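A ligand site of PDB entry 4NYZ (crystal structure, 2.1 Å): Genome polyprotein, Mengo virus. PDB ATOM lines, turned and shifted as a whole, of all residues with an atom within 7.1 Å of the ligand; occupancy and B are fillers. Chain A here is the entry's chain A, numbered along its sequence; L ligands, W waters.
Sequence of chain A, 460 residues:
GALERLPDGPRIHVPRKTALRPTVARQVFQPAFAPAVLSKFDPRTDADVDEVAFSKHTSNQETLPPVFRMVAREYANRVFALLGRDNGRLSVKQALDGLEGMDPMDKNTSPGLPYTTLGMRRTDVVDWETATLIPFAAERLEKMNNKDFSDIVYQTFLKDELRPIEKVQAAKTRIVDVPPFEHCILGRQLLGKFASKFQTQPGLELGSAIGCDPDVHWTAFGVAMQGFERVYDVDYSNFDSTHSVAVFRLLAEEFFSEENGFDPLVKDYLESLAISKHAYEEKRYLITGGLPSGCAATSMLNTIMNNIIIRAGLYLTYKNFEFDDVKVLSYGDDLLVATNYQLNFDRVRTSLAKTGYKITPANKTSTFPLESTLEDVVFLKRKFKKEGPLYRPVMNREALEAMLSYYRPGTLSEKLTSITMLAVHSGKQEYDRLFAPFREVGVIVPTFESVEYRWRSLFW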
ATOM      1  N   LYS A  56      -7.901  -3.797   1.400  1.00  0.00           N
ATOM      2  CA  LYS A  56      -6.503  -3.444   1.161  1.00  0.00           C
ATOM      3  C   LYS A  56      -6.327  -2.398   0.058  1.00  0.00           C
ATOM      4  O   LYS A  56      -5.370  -1.630   0.078  1.00  0.00           O
ATOM      5  CB  LYS A  56      -5.678  -4.698   0.826  1.00  0.00           C
ATOM      6  CG  LYS A  56      -5.915  -5.274  -0.570  1.00  0.00           C
ATOM      7  CD  LYS A  56      -5.005  -6.452  -0.865  1.00  0.00           C
ATOM      8  CE  LYS A  56      -5.701  -7.792  -0.686  1.00  0.00           C
ATOM      9  NZ  LYS A  56      -6.104  -8.066   0.716  1.00  0.00           N
ATOM     10  N   HIS A  57      -7.252  -2.396  -0.908  1.00  0.00           N
ATOM     11  CA  HIS A  57      -7.166  -1.499  -2.063  1.00  0.00           C
ATOM     12  C   HIS A  57      -7.767  -0.105  -1.819  1.00  0.00           C
ATOM     13  O   HIS A  57      -7.721   0.742  -2.698  1.00  0.00           O
ATOM     14  CB  HIS A  57      -7.859  -2.128  -3.275  1.00  0.00           C
ATOM     15  CG  HIS A  57      -7.259  -3.432  -3.697  1.00  0.00           C
ATOM     16  ND1 HIS A  57      -5.987  -3.548  -4.193  1.00  0.00           N
ATOM     17  CD2 HIS A  57      -7.781  -4.687  -3.716  1.00  0.00           C
ATOM     18  CE1 HIS A  57      -5.737  -4.808  -4.494  1.00  0.00           C
ATOM     19  NE2 HIS A  57      -6.809  -5.523  -4.210  1.00  0.00           N
ATOM     20  N   TYR A 236       7.484 -10.089   3.541  1.00  0.00           N
ATOM     21  CA  TYR A 236       6.741  -8.932   3.047  1.00  0.00           C
ATOM     22  C   TYR A 236       5.227  -9.153   3.002  1.00  0.00           C
ATOM     23  O   TYR A 236       4.469  -8.204   2.766  1.00  0.00           O
ATOM     24  CB  TYR A 236       7.207  -8.570   1.632  1.00  0.00           C
ATOM     25  CG  TYR A 236       8.467  -7.749   1.562  1.00  0.00           C
ATOM     26  CD1 TYR A 236       8.417  -6.355   1.558  1.00  0.00           C
ATOM     27  CD2 TYR A 236       9.716  -8.350   1.467  1.00  0.00           C
ATOM     28  CE1 TYR A 236       9.571  -5.589   1.469  1.00  0.00           C
ATOM     29  CE2 TYR A 236      10.873  -7.606   1.383  1.00  0.00           C
ATOM     30  CZ  TYR A 236      10.797  -6.229   1.382  1.00  0.00           C
ATOM     31  OH  TYR A 236      11.953  -5.485   1.298  1.00  0.00           O
ATOM     32  N   SER A 237       4.768 -10.387   3.198  1.00  0.00           N
ATOM     33  CA  SER A 237       3.355 -10.691   3.011  1.00  0.00           C
ATOM     34  C   SER A 237       2.507  -9.835   3.949  1.00  0.00           C
ATOM     35  O   SER A 237       2.780  -9.736   5.139  1.00  0.00           O
ATOM     36  CB  SER A 237       3.061 -12.190   3.228  1.00  0.00           C
ATOM     37  OG  SER A 237       3.323 -12.564   4.563  1.00  0.00           O
ATOM     38  N   ASN A 238       1.512  -9.172   3.370  1.00  0.00           N
ATOM     39  CA  ASN A 238       0.661  -8.256   4.123  1.00  0.00           C
ATOM     40  C   ASN A 238      -0.692  -8.177   3.448  1.00  0.00           C
ATOM     41  O   ASN A 238      -0.818  -7.665   2.335  1.00  0.00           O
ATOM     42  CB  ASN A 238       1.315  -6.868   4.180  1.00  0.00           C
ATOM     43  CG  ASN A 238       0.527  -5.860   5.016  1.00  0.00           C
ATOM     44  OD1 ASN A 238       0.597  -4.658   4.766  1.00  0.00           O
ATOM     45  ND2 ASN A 238      -0.208  -6.330   6.013  1.00  0.00           N
ATOM     46  N   PHE A 239      -1.709  -8.715   4.112  1.00  0.00           N
ATOM     47  CA  PHE A 239      -3.053  -8.752   3.568  1.00  0.00           C
ATOM     48  C   PHE A 239      -3.652  -7.359   3.422  1.00  0.00           C
ATOM     49  O   PHE A 239      -4.419  -7.112   2.505  1.00  0.00           O
ATOM     50  CB  PHE A 239      -3.958  -9.616   4.462  1.00  0.00           C
ATOM     51  CG  PHE A 239      -5.279  -9.955   3.839  1.00  0.00           C
ATOM     52  CD1 PHE A 239      -5.390 -11.029   2.968  1.00  0.00           C
ATOM     53  CD2 PHE A 239      -6.403  -9.210   4.129  1.00  0.00           C
ATOM     54  CE1 PHE A 239      -6.605 -11.352   2.393  1.00  0.00           C
ATOM     55  CE2 PHE A 239      -7.627  -9.524   3.560  1.00  0.00           C
ATOM     56  CZ  PHE A 239      -7.727 -10.593   2.682  1.00  0.00           C
ATOM     57  N   ASP A 240      -3.269  -6.438   4.315  1.00  0.00           N
ATOM     58  CA  ASP A 240      -3.899  -5.128   4.410  1.00  0.00           C
ATOM     59  C   ASP A 240      -3.367  -4.064   3.438  1.00  0.00           C
ATOM     60  O   ASP A 240      -3.932  -2.979   3.359  1.00  0.00           O
ATOM     61  CB  ASP A 240      -3.795  -4.591   5.839  1.00  0.00           C
ATOM     62  CG  ASP A 240      -4.370  -5.553   6.874  1.00  0.00           C
ATOM     63  OD1 ASP A 240      -5.303  -6.309   6.547  1.00  0.00           O
ATOM     64  OD2 ASP A 240      -3.868  -5.550   8.016  1.00  0.00           O
ATOM     65  N   SER A 241      -2.293  -4.351   2.713  1.00  0.00           N
ATOM     66  CA  SER A 241      -1.709  -3.345   1.825  1.00  0.00           C
ATOM     67  C   SER A 241      -1.110  -3.950   0.554  1.00  0.00           C
ATOM     68  O   SER A 241      -0.900  -5.158   0.466  1.00  0.00           O
ATOM     69  CB  SER A 241      -0.637  -2.546   2.565  1.00  0.00           C
ATOM     70  OG  SER A 241      -0.309  -1.367   1.853  1.00  0.00           O
ATOM     71  N   THR A 242      -0.854  -3.077  -0.423  1.00  0.00           N
ATOM     72  CA  THR A 242      -0.299  -3.489  -1.712  1.00  0.00           C
ATOM     73  C   THR A 242       0.840  -2.570  -2.137  1.00  0.00           C
ATOM     74  O   THR A 242       1.125  -1.577  -1.457  1.00  0.00           O
ATOM     75  CB  THR A 242      -1.372  -3.490  -2.809  1.00  0.00           C
ATOM     76  OG1 THR A 242      -1.820  -2.147  -3.041  1.00  0.00           O
ATOM     77  CG2 THR A 242      -2.556  -4.370  -2.430  1.00  0.00           C
ATOM     78  N   HIS A 243       1.487  -2.891  -3.245  1.00  0.00           N
ATOM     79  CA  HIS A 243       2.608  -2.093  -3.742  1.00  0.00           C
ATOM     80  C   HIS A 243       2.163  -0.688  -4.135  1.00  0.00           C
ATOM     81  O   HIS A 243       1.106  -0.500  -4.730  1.00  0.00           O
ATOM     82  CB  HIS A 243       3.286  -2.754  -4.941  1.00  0.00           C
ATOM     83  CG  HIS A 243       4.322  -3.750  -4.570  1.00  0.00           C
ATOM     84  ND1 HIS A 243       4.201  -5.094  -4.835  1.00  0.00           N
ATOM     85  CD2 HIS A 243       5.510  -3.610  -3.930  1.00  0.00           C
ATOM     86  CE1 HIS A 243       5.260  -5.733  -4.388  1.00  0.00           C
ATOM     87  NE2 HIS A 243       6.075  -4.851  -3.824  1.00  0.00           N
ATOM     88  N   SER A 244       2.999   0.282  -3.785  1.00  0.00           N
ATOM     89  CA  SER A 244       2.794   1.665  -4.192  1.00  0.00           C
ATOM     90  C   SER A 244       2.699   1.766  -5.708  1.00  0.00           C
ATOM     91  O   SER A 244       3.428   1.097  -6.442  1.00  0.00           O
ATOM     92  CB  SER A 244       3.964   2.529  -3.697  1.00  0.00           C
ATOM     93  OG  SER A 244       3.832   3.866  -4.144  1.00  0.00           O
ATOM     94  N   PHE A 248       5.765   1.175  -9.538  1.00  0.00           N
ATOM     95  CA  PHE A 248       5.632   0.797 -10.941  1.00  0.00           C
ATOM     96  C   PHE A 248       6.312   1.805 -11.858  1.00  0.00           C
ATOM     97  O   PHE A 248       6.978   1.432 -12.819  1.00  0.00           O
ATOM     98  CB  PHE A 248       4.160   0.661 -11.331  1.00  0.00           C
ATOM     99  CG  PHE A 248       3.485  -0.545 -10.756  1.00  0.00           C
ATOM    100  CD1 PHE A 248       2.846  -0.486  -9.524  1.00  0.00           C
ATOM    101  CD2 PHE A 248       3.470  -1.745 -11.450  1.00  0.00           C
ATOM    102  CE1 PHE A 248       2.222  -1.597  -8.990  1.00  0.00           C
ATOM    103  CE2 PHE A 248       2.849  -2.858 -10.925  1.00  0.00           C
ATOM    104  CZ  PHE A 248       2.222  -2.794  -9.700  1.00  0.00           C
ATOM    105  N   GLY A 289      -2.613   1.060  -7.781  1.00  0.00           N
ATOM    106  CA  GLY A 289      -1.559   0.325  -7.103  1.00  0.00           C
ATOM    107  C   GLY A 289      -1.885  -1.155  -7.031  1.00  0.00           C
ATOM    108  O   GLY A 289      -2.988  -1.584  -7.404  1.00  0.00           O
ATOM    109  N   GLY A 290      -0.923  -1.941  -6.563  1.00  0.00           N
ATOM    110  CA  GLY A 290      -1.095  -3.380  -6.461  1.00  0.00           C
ATOM    111  C   GLY A 290      -0.714  -4.099  -7.740  1.00  0.00           C
ATOM    112  O   GLY A 290      -0.771  -3.532  -8.836  1.00  0.00           O
ATOM    113  N   LEU A 291      -0.332  -5.353  -7.581  1.00  0.00           N
ATOM    114  CA  LEU A 291       0.162  -6.194  -8.666  1.00  0.00           C
ATOM    115  C   LEU A 291      -0.899  -7.261  -8.944  1.00  0.00           C
ATOM    116  O   LEU A 291      -1.321  -7.959  -8.016  1.00  0.00           O
ATOM    117  CB  LEU A 291       1.477  -6.832  -8.210  1.00  0.00           C
ATOM    118  CG  LEU A 291       2.576  -7.217  -9.201  1.00  0.00           C
ATOM    119  CD1 LEU A 291       2.994  -6.067 -10.090  1.00  0.00           C
ATOM    120  CD2 LEU A 291       3.782  -7.720  -8.409  1.00  0.00           C
ATOM    121  N   PRO A 292      -1.371  -7.369 -10.196  1.00  0.00           N
ATOM    122  CA  PRO A 292      -2.322  -8.452 -10.506  1.00  0.00           C
ATOM    123  C   PRO A 292      -1.675  -9.829 -10.398  1.00  0.00           C
ATOM    124  O   PRO A 292      -0.517  -9.999 -10.777  1.00  0.00           O
ATOM    125  CB  PRO A 292      -2.738  -8.159 -11.960  1.00  0.00           C
ATOM    126  CG  PRO A 292      -2.404  -6.725 -12.183  1.00  0.00           C
ATOM    127  CD  PRO A 292      -1.196  -6.458 -11.341  1.00  0.00           C
ATOM    128  N   SER A 293      -2.420 -10.808  -9.901  1.00  0.00           N
ATOM    129  CA  SER A 293      -1.877 -12.130  -9.594  1.00  0.00           C
ATOM    130  C   SER A 293      -1.627 -13.011 -10.829  1.00  0.00           C
ATOM    131  O   SER A 293      -0.582 -13.643 -10.941  1.00  0.00           O
ATOM    132  CB  SER A 293      -2.807 -12.867  -8.635  1.00  0.00           C
ATOM    133  OG  SER A 293      -4.049 -13.141  -9.260  1.00  0.00           O
ATOM    134  N   THR A 298       4.222 -11.479 -12.597  1.00  0.00           N
ATOM    135  CA  THR A 298       3.902 -11.042 -11.234  1.00  0.00           C
ATOM    136  C   THR A 298       5.009 -11.322 -10.216  1.00  0.00           C
ATOM    137  O   THR A 298       5.508 -10.392  -9.574  1.00  0.00           O
ATOM    138  CB  THR A 298       2.601 -11.699 -10.721  1.00  0.00           C
ATOM    139  OG1 THR A 298       1.540 -11.453 -11.652  1.00  0.00           O
ATOM    140  CG2 THR A 298       2.210 -11.161  -9.339  1.00  0.00           C
ATOM    141  N   ASN A 302       7.355  -8.624  -8.332  1.00  0.00           N
ATOM    142  CA  ASN A 302       7.305  -8.591  -6.873  1.00  0.00           C
ATOM    143  C   ASN A 302       8.688  -8.834  -6.266  1.00  0.00           C
ATOM    144  O   ASN A 302       9.101  -8.125  -5.346  1.00  0.00           O
ATOM    145  CB  ASN A 302       6.313  -9.640  -6.359  1.00  0.00           C
ATOM    146  CG  ASN A 302       6.059  -9.525  -4.861  1.00  0.00           C
ATOM    147  OD1 ASN A 302       6.239  -8.472  -4.263  1.00  0.00           O
ATOM    148  ND2 ASN A 302       5.636 -10.633  -4.252  1.00  0.00           N
ATOM    149  N   MET A 305      10.953  -5.730  -6.910  1.00  0.00           N
ATOM    150  CA  MET A 305      10.499  -4.626  -6.052  1.00  0.00           C
ATOM    151  C   MET A 305      10.956  -4.819  -4.610  1.00  0.00           C
ATOM    152  O   MET A 305      11.512  -3.902  -3.999  1.00  0.00           O
ATOM    153  CB  MET A 305       8.974  -4.525  -6.081  1.00  0.00           C
ATOM    154  CG  MET A 305       8.419  -3.928  -7.359  1.00  0.00           C
ATOM    155  SD  MET A 305       6.614  -3.852  -7.327  1.00  0.00           S
ATOM    156  CE  MET A 305       6.276  -3.150  -8.943  1.00  0.00           C
ATOM    157  N   ASN A 306      10.751  -6.017  -4.077  1.00  0.00           N
ATOM    158  CA  ASN A 306      11.079  -6.309  -2.689  1.00  0.00           C
ATOM    159  C   ASN A 306      12.597  -6.310  -2.419  1.00  0.00           C
ATOM    160  O   ASN A 306      13.028  -5.994  -1.305  1.00  0.00           O
ATOM    161  CB  ASN A 306      10.450  -7.632  -2.249  1.00  0.00           C
ATOM    162  CG  ASN A 306       8.930  -7.556  -2.164  1.00  0.00           C
ATOM    163  OD1 ASN A 306       8.346  -6.478  -2.141  1.00  0.00           O
ATOM    164  ND2 ASN A 306       8.286  -8.714  -2.095  1.00  0.00           N
ATOM    165  N   GLY A 332       9.525 -13.504  -4.371  1.00  0.00           N
ATOM    166  CA  GLY A 332       8.210 -12.958  -4.032  1.00  0.00           C
ATOM    167  C   GLY A 332       8.287 -12.205  -2.716  1.00  0.00           C
ATOM    168  O   GLY A 332       9.092 -11.281  -2.575  1.00  0.00           O
ATOM    169  N   ASP A 333       7.470 -12.628  -1.748  1.00  0.00           N
ATOM    170  CA  ASP A 333       7.397 -11.999  -0.423  1.00  0.00           C
ATOM    171  C   ASP A 333       8.441 -12.509   0.580  1.00  0.00           C
ATOM    172  O   ASP A 333       8.537 -11.977   1.682  1.00  0.00           O
ATOM    173  CB  ASP A 333       6.002 -12.204   0.181  1.00  0.00           C
ATOM    174  CG  ASP A 333       4.931 -11.351  -0.492  1.00  0.00           C
ATOM    175  OD1 ASP A 333       5.280 -10.393  -1.211  1.00  0.00           O
ATOM    176  OD2 ASP A 333       3.737 -11.642  -0.285  1.00  0.00           O
ATOM    177  N   GLY A 356       4.623   3.053   3.824  1.00  0.00           N
ATOM    178  CA  GLY A 356       3.526   2.128   3.606  1.00  0.00           C
ATOM    179  C   GLY A 356       3.890   0.647   3.505  1.00  0.00           C
ATOM    180  O   GLY A 356       3.021  -0.178   3.247  1.00  0.00           O
ATOM    181  N   TYR A 357       5.161   0.306   3.708  1.00  0.00           N
ATOM    182  CA  TYR A 357       5.606  -1.086   3.568  1.00  0.00           C
ATOM    183  C   TYR A 357       5.821  -1.761   4.906  1.00  0.00           C
ATOM    184  O   TYR A 357       6.503  -1.233   5.785  1.00  0.00           O
ATOM    185  CB  TYR A 357       6.888  -1.161   2.733  1.00  0.00           C
ATOM    186  CG  TYR A 357       6.630  -1.042   1.250  1.00  0.00           C
ATOM    187  CD1 TYR A 357       6.066  -2.105   0.553  1.00  0.00           C
ATOM    188  CD2 TYR A 357       6.916   0.116   0.559  1.00  0.00           C
ATOM    189  CE1 TYR A 357       5.814  -2.017  -0.803  1.00  0.00           C
ATOM    190  CE2 TYR A 357       6.674   0.224  -0.797  1.00  0.00           C
ATOM    191  CZ  TYR A 357       6.117  -0.837  -1.470  1.00  0.00           C
ATOM    192  OH  TYR A 357       5.877  -0.735  -2.813  1.00  0.00           O
ATOM    193  N   LYS A 358       5.233  -2.950   5.055  1.00  0.00           N
ATOM    194  CA  LYS A 358       5.344  -3.752   6.267  1.00  0.00           C
ATOM    195  C   LYS A 358       6.319  -4.904   6.047  1.00  0.00           C
ATOM    196  O   LYS A 358       6.207  -5.629   5.059  1.00  0.00           O
ATOM    197  CB  LYS A 358       3.976  -4.308   6.672  1.00  0.00           C
ATOM    198  CG  LYS A 358       3.987  -5.190   7.914  1.00  0.00           C
ATOM    199  CD  LYS A 358       2.593  -5.668   8.274  1.00  0.00           C
ATOM    200  CE  LYS A 358       2.619  -6.601   9.466  1.00  0.00           C
ATOM    201  NZ  LYS A 358       1.300  -7.241   9.720  1.00  0.00           N
HETATM  202  N1  LIG L   1       3.931  -8.062  -0.830  1.00  0.00           N
HETATM  203  C1  LIG L   1       2.923  -7.005  -1.136  1.00  0.00           C
HETATM  204  C2  LIG L   1       2.042  -6.683   0.078  1.00  0.00           C
HETATM  205  O1  LIG L   1       0.888  -7.107   0.183  1.00  0.00           O
HETATM  206  C3  LIG L   1       2.055  -7.420  -2.321  1.00  0.00           C
HETATM  207  C4  LIG L   1       1.141  -6.313  -2.807  1.00  0.00           C
HETATM  208  C5  LIG L   1       0.724  -6.465  -4.248  1.00  0.00           C
HETATM  209  O2  LIG L   1       1.109  -5.680  -5.096  1.00  0.00           O
HETATM  210  N2  LIG L   1      -0.079  -7.483  -4.523  1.00  0.00           N
HETATM  211  O3  LIG L   1       2.487  -5.974   0.977  1.00  0.00           O
HETATM  212  O   HOH W   1       1.840 -10.719  -2.072  1.00  0.00           O
HETATM  213  O   HOH W   2      -2.523  -7.747  -3.405  1.00  0.00           O
HETATM  214  O   HOH W   3       5.036  -5.548   2.470  1.00  0.00           O
HETATM  215  O   HOH W   4      -1.580  -8.215  -0.693  1.00  0.00           O
HETATM  216  O   HOH W   5       1.814  -9.520  -4.848  1.00  0.00           O
HETATM  217  O   HOH W   6       3.108  -3.745   3.170  1.00  0.00           O
HETATM  218  O   HOH W   7       0.772  -9.848   0.611  1.00  0.00           O
HETATM  219  O   HOH W   8       5.843  -5.853  -0.724  1.00  0.00           O
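The backbone carbonyl oxygen (O) of Ser 241 sits close to an oxygen (O1) of the ligand (2.7 Å).
N1 of the ligand lies within salt-bridge range of OD1 of Asp 333.
An oxygen (O1) of the ligand lies close to the backbone carbonyl oxygen (O) of Asn 238 (2.8 Å).
The backbone NH of Leu 291 lies within hydrogen-bond range of an oxygen (O2) of the ligand, 2.9 Å away.
The backbone NH (N) of His 243 lies within hydrogen-bond range of an oxygen (O2) of the ligand, 3.4 Å away.
A ring nitrogen (ND1) of His 243 lies within hydrogen-bond range of an oxygen (O2) of the ligand, 3.2 Å away.
N of Tyr 236 lies within hydrogen-bond range of O of Asp 333, at 2.9 Å.
The side-chain amide nitrogen (ND2) of Asn 302 sits at hydrogen-bond distance from the side-chain carboxylate (OD1) of Asp 333 (3.1 Å).
The backbone carbonyl oxygen (O) of His 243 sits at hydrogen-bond distance from the backbone NH (N) of Gly 290 (3.1 Å).
The side-chain amide oxygen (OD1) of Asn 306 lies within hydrogen-bond range of a ring nitrogen (NE2) of His 243, at 3.3 Å.
A ring nitrogen (NE2) of His 243 sits close to the side-chain sulfur of Met 305, at 3.7 Å.
The backbone carbonyl oxygen (O) of Asn 306 lies within hydrogen-bond range of the side-chain hydroxyl (OH) of Tyr 236, at 2.9 Å.
An oxygen (O3) of the ligand sits close to the backbone carbonyl oxygen of Tyr 236, 3.5 Å away.
Residues that only touch the ligand: Thr 242 and Gly 290.
Of the 26 residues printed, 8 come within 4 Å of the ligand.
The nearest printed residue that does not touch the ligand is Asn 302 (4.2 Å).
Water W7 lies within hydrogen-bond range of O1 of the ligand (2.8 Å) and N of Asn 238 (2.9 Å).
Water W4 lies within hydrogen-bond range of an oxygen (O1) of the ligand (2.8 Å), the backbone carbonyl oxygen of Asn 238 (3.2 Å) and the backbone carbonyl oxygen of Ser 241 (3.3 Å).
Water W8 lies within hydrogen-bond range of a nitrogen (N1) of the ligand (2.9 Å), the side-chain amide oxygen of Asn 306 (2.9 Å) and a ring nitrogen (NE2) of His 243 (3.3 Å).
Water W3 lies within hydrogen-bond range of O of Tyr 236 (2.7 Å), O of Lys 358 (2.8 Å) and O3 of the ligand (3.0 Å).
Water W6 lies within hydrogen-bond range of N of Lys 358, OD1 of Asn 238 and O3 of the ligand.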
